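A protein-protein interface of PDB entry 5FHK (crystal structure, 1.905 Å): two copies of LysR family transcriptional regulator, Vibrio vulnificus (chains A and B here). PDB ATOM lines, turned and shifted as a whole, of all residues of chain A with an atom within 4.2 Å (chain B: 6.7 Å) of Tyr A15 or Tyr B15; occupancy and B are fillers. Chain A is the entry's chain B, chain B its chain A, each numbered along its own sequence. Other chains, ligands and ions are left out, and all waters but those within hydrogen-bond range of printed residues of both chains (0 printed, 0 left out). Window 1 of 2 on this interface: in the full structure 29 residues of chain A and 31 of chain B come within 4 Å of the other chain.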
ATOM      1  N   THR A  13      14.533  -4.249  14.819  1.00  0.00           N
ATOM      2  CA  THR A  13      15.435  -3.543  13.919  1.00  0.00           C
ATOM      3  C   THR A  13      16.261  -4.514  13.089  1.00  0.00           C
ATOM      4  O   THR A  13      16.482  -5.655  13.503  1.00  0.00           O
ATOM      5  CB  THR A  13      16.378  -2.599  14.695  1.00  0.00           C
ATOM      6  OG1 THR A  13      17.236  -3.345  15.564  1.00  0.00           O
ATOM      7  CG2 THR A  13      15.567  -1.587  15.537  1.00  0.00           C
ATOM      8  N   PRO A  14      16.745  -4.081  11.920  1.00  0.00           N
ATOM      9  CA  PRO A  14      17.509  -4.988  11.055  1.00  0.00           C
ATOM     10  C   PRO A  14      18.780  -5.464  11.740  1.00  0.00           C
ATOM     11  O   PRO A  14      19.532  -4.676  12.309  1.00  0.00           O
ATOM     12  CB  PRO A  14      17.831  -4.125   9.827  1.00  0.00           C
ATOM     13  CG  PRO A  14      16.840  -2.993   9.871  1.00  0.00           C
ATOM     14  CD  PRO A  14      16.600  -2.743  11.319  1.00  0.00           C
ATOM     15  N   TYR A  15      19.033  -6.766  11.648  1.00  0.00           N
ATOM     16  CA  TYR A  15      20.019  -7.373  12.530  1.00  0.00           C
ATOM     17  C   TYR A  15      21.437  -6.882  12.245  1.00  0.00           C
ATOM     18  O   TYR A  15      22.222  -6.681  13.181  1.00  0.00           O
ATOM     19  CB  TYR A  15      19.962  -8.888  12.434  1.00  0.00           C
ATOM     20  CG  TYR A  15      21.136  -9.485  13.133  1.00  0.00           C
ATOM     21  CD1 TYR A  15      21.225  -9.442  14.514  1.00  0.00           C
ATOM     22  CD2 TYR A  15      22.187 -10.039  12.419  1.00  0.00           C
ATOM     23  CE1 TYR A  15      22.317  -9.965  15.170  1.00  0.00           C
ATOM     24  CE2 TYR A  15      23.286 -10.571  13.068  1.00  0.00           C
ATOM     25  CZ  TYR A  15      23.346 -10.531  14.444  1.00  0.00           C
ATOM     26  OH  TYR A  15      24.436 -11.055  15.099  1.00  0.00           O
ATOM     27  N   ASN A  16      21.801  -6.703  10.975  1.00  0.00           N
ATOM     28  CA  ASN A  16      23.172  -6.279  10.686  1.00  0.00           C
ATOM     29  C   ASN A  16      23.348  -4.765  10.746  1.00  0.00           C
ATOM     30  O   ASN A  16      24.438  -4.283  11.086  1.00  0.00           O
ATOM     31  CB  ASN A  16      23.606  -6.792   9.315  1.00  0.00           C
ATOM     32  CG  ASN A  16      24.048  -8.242   9.352  1.00  0.00           C
ATOM     33  OD1 ASN A  16      24.905  -8.622  10.151  1.00  0.00           O
ATOM     34  ND2 ASN A  16      23.445  -9.065   8.498  1.00  0.00           N
ATOM     35  N   LEU A  17      22.302  -4.003  10.446  1.00  0.00           N
ATOM     36  CA  LEU A  17      22.413  -2.569  10.276  1.00  0.00           C
ATOM     37  C   LEU A  17      22.168  -1.771  11.553  1.00  0.00           C
ATOM     38  O   LEU A  17      22.305  -0.544  11.523  1.00  0.00           O
ATOM     39  CB  LEU A  17      21.420  -2.115   9.202  1.00  0.00           C
ATOM     40  CG  LEU A  17      21.390  -3.006   7.964  1.00  0.00           C
ATOM     41  CD1 LEU A  17      20.226  -2.699   7.051  1.00  0.00           C
ATOM     42  CD2 LEU A  17      22.698  -2.860   7.211  1.00  0.00           C
ATOM     43  N   THR A  42      17.142  -6.998  17.826  1.00  0.00           N
ATOM     44  CA  THR A  42      17.669  -7.124  16.476  1.00  0.00           C
ATOM     45  C   THR A  42      17.129  -8.404  15.852  1.00  0.00           C
ATOM     46  O   THR A  42      17.103  -9.458  16.499  1.00  0.00           O
ATOM     47  CB  THR A  42      19.192  -7.123  16.486  1.00  0.00           C
ATOM     48  OG1 THR A  42      19.656  -8.183  17.323  1.00  0.00           O
ATOM     49  CG2 THR A  42      19.715  -5.793  16.999  1.00  0.00           C
ATOM     50  N   GLU A  43      16.660  -8.304  14.607  1.00  0.00           N
ATOM     51  CA  GLU A  43      15.941  -9.385  13.943  1.00  0.00           C
ATOM     52  C   GLU A  43      16.515  -9.605  12.552  1.00  0.00           C
ATOM     53  O   GLU A  43      16.629  -8.661  11.766  1.00  0.00           O
ATOM     54  CB  GLU A  43      14.440  -9.074  13.854  1.00  0.00           C
ATOM     55  CG  GLU A  43      13.627 -10.141  13.155  1.00  0.00           C
ATOM     56  CD  GLU A  43      13.707 -11.499  13.847  1.00  0.00           C
ATOM     57  OE1 GLU A  43      14.619 -12.292  13.516  1.00  0.00           O
ATOM     58  OE2 GLU A  43      12.846 -11.778  14.715  1.00  0.00           O
ATOM     59  N   SER A  44      16.865 -10.859  12.252  1.00  0.00           N
ATOM     60  CA  SER A  44      17.424 -11.205  10.950  1.00  0.00           C
ATOM     61  C   SER A  44      16.368 -11.227   9.854  1.00  0.00           C
ATOM     62  O   SER A  44      16.678 -10.928   8.694  1.00  0.00           O
ATOM     63  CB  SER A  44      18.115 -12.566  11.019  1.00  0.00           C
ATOM     64  OG  SER A  44      18.897 -12.797   9.861  1.00  0.00           O
ATOM     65  N   ASN A 134      27.064 -16.282  10.257  1.00  0.00           N
ATOM     66  CA  ASN A 134      25.702 -15.802  10.399  1.00  0.00           C
ATOM     67  C   ASN A 134      25.642 -14.337  10.800  1.00  0.00           C
ATOM     68  O   ASN A 134      24.553 -13.832  11.068  1.00  0.00           O
ATOM     69  CB  ASN A 134      24.933 -16.662  11.409  1.00  0.00           C
ATOM     70  CG  ASN A 134      25.490 -16.569  12.826  1.00  0.00           C
ATOM     71  OD1 ASN A 134      26.714 -16.500  13.047  1.00  0.00           O
ATOM     72  ND2 ASN A 134      24.591 -16.574  13.801  1.00  0.00           N
ATOM     73  N   ALA A 135      26.779 -13.643  10.824  1.00  0.00           N
ATOM     74  CA  ALA A 135      26.833 -12.219  11.137  1.00  0.00           C
ATOM     75  C   ALA A 135      27.828 -11.541  10.214  1.00  0.00           C
ATOM     76  O   ALA A 135      28.906 -12.080   9.957  1.00  0.00           O
ATOM     77  CB  ALA A 135      27.246 -11.973  12.592  1.00  0.00           C
ATOM     78  N   THR B  13      30.428 -20.293  18.301  1.00  0.00           N
ATOM     79  CA  THR B  13      31.111 -19.337  19.167  1.00  0.00           C
ATOM     80  C   THR B  13      30.089 -18.461  19.890  1.00  0.00           C
ATOM     81  O   THR B  13      28.979 -18.262  19.383  1.00  0.00           O
ATOM     82  CB  THR B  13      32.059 -18.428  18.369  1.00  0.00           C
ATOM     83  OG1 THR B  13      31.286 -17.687  17.414  1.00  0.00           O
ATOM     84  CG2 THR B  13      33.129 -19.254  17.643  1.00  0.00           C
ATOM     85  N   PRO B  14      30.440 -17.921  21.069  1.00  0.00           N
ATOM     86  CA  PRO B  14      29.465 -17.157  21.871  1.00  0.00           C
ATOM     87  C   PRO B  14      29.112 -15.803  21.265  1.00  0.00           C
ATOM     88  O   PRO B  14      29.955 -15.116  20.682  1.00  0.00           O
ATOM     89  CB  PRO B  14      30.179 -16.971  23.218  1.00  0.00           C
ATOM     90  CG  PRO B  14      31.623 -17.126  22.911  1.00  0.00           C
ATOM     91  CD  PRO B  14      31.686 -18.162  21.818  1.00  0.00           C
ATOM     92  N   TYR B  15      27.853 -15.401  21.472  1.00  0.00           N
ATOM     93  CA  TYR B  15      27.261 -14.326  20.670  1.00  0.00           C
ATOM     94  C   TYR B  15      28.058 -13.015  20.754  1.00  0.00           C
ATOM     95  O   TYR B  15      28.585 -12.519  19.744  1.00  0.00           O
ATOM     96  CB  TYR B  15      25.808 -14.111  21.078  1.00  0.00           C
ATOM     97  CG  TYR B  15      25.161 -13.049  20.235  1.00  0.00           C
ATOM     98  CD1 TYR B  15      25.417 -12.978  18.870  1.00  0.00           C
ATOM     99  CD2 TYR B  15      24.345 -12.077  20.800  1.00  0.00           C
ATOM    100  CE1 TYR B  15      24.857 -11.985  18.084  1.00  0.00           C
ATOM    101  CE2 TYR B  15      23.786 -11.085  20.022  1.00  0.00           C
ATOM    102  CZ  TYR B  15      24.046 -11.048  18.664  1.00  0.00           C
ATOM    103  OH  TYR B  15      23.494 -10.062  17.877  1.00  0.00           O
ATOM    104  N   ASN B  16      28.183 -12.450  21.946  1.00  0.00           N
ATOM    105  CA  ASN B  16      28.718 -11.090  22.055  1.00  0.00           C
ATOM    106  C   ASN B  16      30.233 -10.987  21.968  1.00  0.00           C
ATOM    107  O   ASN B  16      30.743  -9.873  21.787  1.00  0.00           O
ATOM    108  CB  ASN B  16      28.294 -10.468  23.368  1.00  0.00           C
ATOM    109  CG  ASN B  16      26.837 -10.177  23.406  1.00  0.00           C
ATOM    110  OD1 ASN B  16      26.343  -9.367  22.628  1.00  0.00           O
ATOM    111  ND2 ASN B  16      26.129 -10.816  24.326  1.00  0.00           N
ATOM    112  N   LEU B  17      30.962 -12.099  22.088  1.00  0.00           N
ATOM    113  CA  LEU B  17      32.401 -12.071  22.290  1.00  0.00           C
ATOM    114  C   LEU B  17      33.180 -12.505  21.070  1.00  0.00           C
ATOM    115  O   LEU B  17      34.413 -12.442  21.088  1.00  0.00           O
ATOM    116  CB  LEU B  17      32.788 -12.991  23.459  1.00  0.00           C
ATOM    117  CG  LEU B  17      32.101 -12.773  24.805  1.00  0.00           C
ATOM    118  CD1 LEU B  17      32.549 -13.859  25.775  1.00  0.00           C
ATOM    119  CD2 LEU B  17      32.464 -11.416  25.357  1.00  0.00           C
ATOM    120  N   THR B  18      32.502 -12.966  20.023  1.00  0.00           N
ATOM    121  CA  THR B  18      33.192 -13.602  18.905  1.00  0.00           C
ATOM    122  C   THR B  18      34.165 -12.653  18.236  1.00  0.00           C
ATOM    123  O   THR B  18      35.318 -13.013  17.974  1.00  0.00           O
ATOM    124  CB  THR B  18      32.180 -14.110  17.890  1.00  0.00           C
ATOM    125  OG1 THR B  18      31.551 -15.284  18.411  1.00  0.00           O
ATOM    126  CG2 THR B  18      32.859 -14.425  16.560  1.00  0.00           C
ATOM    127  N   LYS B  19      33.722 -11.431  17.958  1.00  0.00           N
ATOM    128  CA  LYS B  19      34.561 -10.486  17.239  1.00  0.00           C
ATOM    129  C   LYS B  19      35.867 -10.229  17.990  1.00  0.00           C
ATOM    130  O   LYS B  19      36.952 -10.342  17.416  1.00  0.00           O
ATOM    131  CB  LYS B  19      33.781  -9.192  16.992  1.00  0.00           C
ATOM    132  CG  LYS B  19      34.626  -8.102  16.411  1.00  0.00           C
ATOM    133  CD  LYS B  19      34.719  -8.199  14.916  1.00  0.00           C
ATOM    134  CE  LYS B  19      35.539  -7.032  14.396  1.00  0.00           C
ATOM    135  NZ  LYS B  19      36.909  -7.039  15.005  1.00  0.00           N
ATOM    136  N   THR B  42      27.561 -17.605  15.425  1.00  0.00           N
ATOM    137  CA  THR B  42      27.501 -17.034  16.767  1.00  0.00           C
ATOM    138  C   THR B  42      26.261 -17.571  17.482  1.00  0.00           C
ATOM    139  O   THR B  42      25.180 -17.635  16.897  1.00  0.00           O
ATOM    140  CB  THR B  42      27.453 -15.505  16.712  1.00  0.00           C
ATOM    141  OG1 THR B  42      26.177 -15.087  16.228  1.00  0.00           O
ATOM    142  CG2 THR B  42      28.506 -14.944  15.781  1.00  0.00           C
ATOM    143  N   GLU B  43      26.415 -17.955  18.751  1.00  0.00           N
ATOM    144  CA  GLU B  43      25.417 -18.750  19.464  1.00  0.00           C
ATOM    145  C   GLU B  43      25.164 -18.198  20.865  1.00  0.00           C
ATOM    146  O   GLU B  43      26.111 -17.879  21.584  1.00  0.00           O
ATOM    147  CB  GLU B  43      25.891 -20.210  19.565  1.00  0.00           C
ATOM    148  CG  GLU B  43      24.945 -21.120  20.295  1.00  0.00           C
ATOM    149  CD  GLU B  43      23.527 -20.933  19.819  1.00  0.00           C
ATOM    150  OE1 GLU B  43      22.653 -20.652  20.673  1.00  0.00           O
ATOM    151  OE2 GLU B  43      23.304 -21.060  18.585  1.00  0.00           O
ATOM    152  N   SER B  44      23.888 -18.141  21.273  1.00  0.00           N
ATOM    153  CA  SER B  44      23.481 -17.614  22.582  1.00  0.00           C
ATOM    154  C   SER B  44      23.405 -18.673  23.686  1.00  0.00           C
ATOM    155  O   SER B  44      23.925 -18.460  24.786  1.00  0.00           O
ATOM    156  CB  SER B  44      22.126 -16.909  22.475  1.00  0.00           C
ATOM    157  OG  SER B  44      22.248 -15.686  21.772  1.00  0.00           O
ATOM    158  N   VAL B  60      30.765 -19.989  26.530  1.00  0.00           N
ATOM    159  CA  VAL B  60      30.918 -19.422  27.858  1.00  0.00           C
ATOM    160  C   VAL B  60      30.345 -20.412  28.859  1.00  0.00           C
ATOM    161  O   VAL B  60      29.254 -20.960  28.646  1.00  0.00           O
ATOM    162  CB  VAL B  60      30.209 -18.064  27.954  1.00  0.00           C
ATOM    163  CG1 VAL B  60      30.177 -17.582  29.394  1.00  0.00           C
ATOM    164  CG2 VAL B  60      30.891 -17.042  27.057  1.00  0.00           C
ATOM    165  N   HIS B 108      21.385  -8.680  26.657  1.00  0.00           N
ATOM    166  CA  HIS B 108      21.509 -10.125  26.827  1.00  0.00           C
ATOM    167  C   HIS B 108      22.957 -10.550  26.602  1.00  0.00           C
ATOM    168  O   HIS B 108      23.634  -9.994  25.728  1.00  0.00           O
ATOM    169  CB  HIS B 108      20.617 -10.878  25.834  1.00  0.00           C
ATOM    170  CG  HIS B 108      19.177 -10.982  26.237  1.00  0.00           C
ATOM    171  ND1 HIS B 108      18.167 -10.332  25.558  1.00  0.00           N
ATOM    172  CD2 HIS B 108      18.571 -11.700  27.215  1.00  0.00           C
ATOM    173  CE1 HIS B 108      17.003 -10.625  26.113  1.00  0.00           C
ATOM    174  NE2 HIS B 108      17.220 -11.452  27.121  1.00  0.00           N
ATOM    175  N   PRO B 109      23.456 -11.563  27.336  1.00  0.00           N
ATOM    176  CA  PRO B 109      22.787 -12.382  28.356  1.00  0.00           C
ATOM    177  C   PRO B 109      22.963 -11.815  29.767  1.00  0.00           C
ATOM    178  O   PRO B 109      23.015 -12.577  30.735  1.00  0.00           O
ATOM    179  CB  PRO B 109      23.511 -13.725  28.228  1.00  0.00           C
ATOM    180  CG  PRO B 109      24.951 -13.312  27.953  1.00  0.00           C
ATOM    181  CD  PRO B 109      24.852 -12.000  27.135  1.00  0.00           C
ATOM    182  N   ASN B 134      18.860  -7.254  22.960  1.00  0.00           N
ATOM    183  CA  ASN B 134      19.369  -8.620  22.895  1.00  0.00           C
ATOM    184  C   ASN B 134      20.826  -8.706  22.421  1.00  0.00           C
ATOM    185  O   ASN B 134      21.322  -9.819  22.210  1.00  0.00           O
ATOM    186  CB  ASN B 134      18.473  -9.480  21.995  1.00  0.00           C
ATOM    187  CG  ASN B 134      18.331  -8.921  20.589  1.00  0.00           C
ATOM    188  OD1 ASN B 134      18.556  -7.726  20.343  1.00  0.00           O
ATOM    189  ND2 ASN B 134      17.929  -9.782  19.659  1.00  0.00           N
ATOM    190  N   ALA B 135      21.518  -7.577  22.244  1.00  0.00           N
ATOM    191  CA  ALA B 135      22.934  -7.567  21.882  1.00  0.00           C
ATOM    192  C   ALA B 135      23.660  -6.513  22.713  1.00  0.00           C
ATOM    193  O   ALA B 135      23.102  -5.451  22.994  1.00  0.00           O
ATOM    194  CB  ALA B 135      23.148  -7.280  20.381  1.00  0.00           C
ATOM    195  N   LEU B 136      24.922  -6.781  23.066  1.00  0.00           N
ATOM    196  CA  LEU B 136      25.651  -5.876  23.959  1.00  0.00           C
ATOM    197  C   LEU B 136      26.348  -4.743  23.228  1.00  0.00           C
ATOM    198  O   LEU B 136      26.590  -3.687  23.831  1.00  0.00           O
ATOM    199  CB  LEU B 136      26.691  -6.644  24.790  1.00  0.00           C
ATOM    200  CG  LEU B 136      26.097  -7.314  26.048  1.00  0.00           C
ATOM    201  CD1 LEU B 136      27.130  -8.199  26.750  1.00  0.00           C
ATOM    202  CD2 LEU B 136      25.525  -6.296  27.020  1.00  0.00           C
ATOM    203  N   ASN B 137      26.668  -4.926  21.942  1.00  0.00           N
ATOM    204  CA  ASN B 137      27.307  -3.847  21.204  1.00  0.00           C
ATOM    205  C   ASN B 137      26.423  -2.597  21.168  1.00  0.00           C
ATOM    206  O   ASN B 137      26.912  -1.490  21.416  1.00  0.00           O
ATOM    207  CB  ASN B 137      27.697  -4.313  19.792  1.00  0.00           C
ATOM    208  CG  ASN B 137      26.494  -4.700  18.925  1.00  0.00           C
ATOM    209  OD1 ASN B 137      25.409  -5.027  19.426  1.00  0.00           O
ATOM    210  ND2 ASN B 137      26.695  -4.672  17.609  1.00  0.00           N
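Of the 10 printed residues of chain A, 3 touch a printed residue of chain B.
Hydrophobic or aromatic side chains of chain B within 4 Å of the printed part of chain A: Tyr B15.
Among the printed residues, 3 pairs touch across the chains.
OH of Tyr A15 sits close to OH of Tyr B15 (3.1 Å).
N of Thr B42 is in hydrogen-bond range of OD1 of Asn A134 (2.8 Å).
OD1 of Asn B134 is in hydrogen-bond range of N of Thr A42.
N of Tyr B15 lies within hydrogen-bond range of O of Glu B43 (3.0 Å).
N of Tyr A15 sits at hydrogen-bond distance from O of Glu A43 (3.1 Å).
Of chain B, only Tyr B15 comes within 4 Å of Tyr A15.
Of chain A, only Tyr A15 comes within 4 Å of Tyr B15.
Of the printed residues of chain B, Asn A134 touches Thr B42 (2.8 Å).
Printed residues of chain A within 4 Å of Asn B134: Thr A42.
Printed residues of chain B within 4 Å of Thr A42: Asn B134.
Of the printed residues of chain A, Thr B42 touches Asn A134.
Glu B43 touches none of the printed residues of chain A.
The nearest residue of chain B that does not touch Tyr A15 is Thr B42 (4.5 Å).
Tyr A15 touches its own counterpart, Tyr B15.
Thr A42 touches Asn B134, and with the chains exchanged Asn A134 touches Thr B42.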
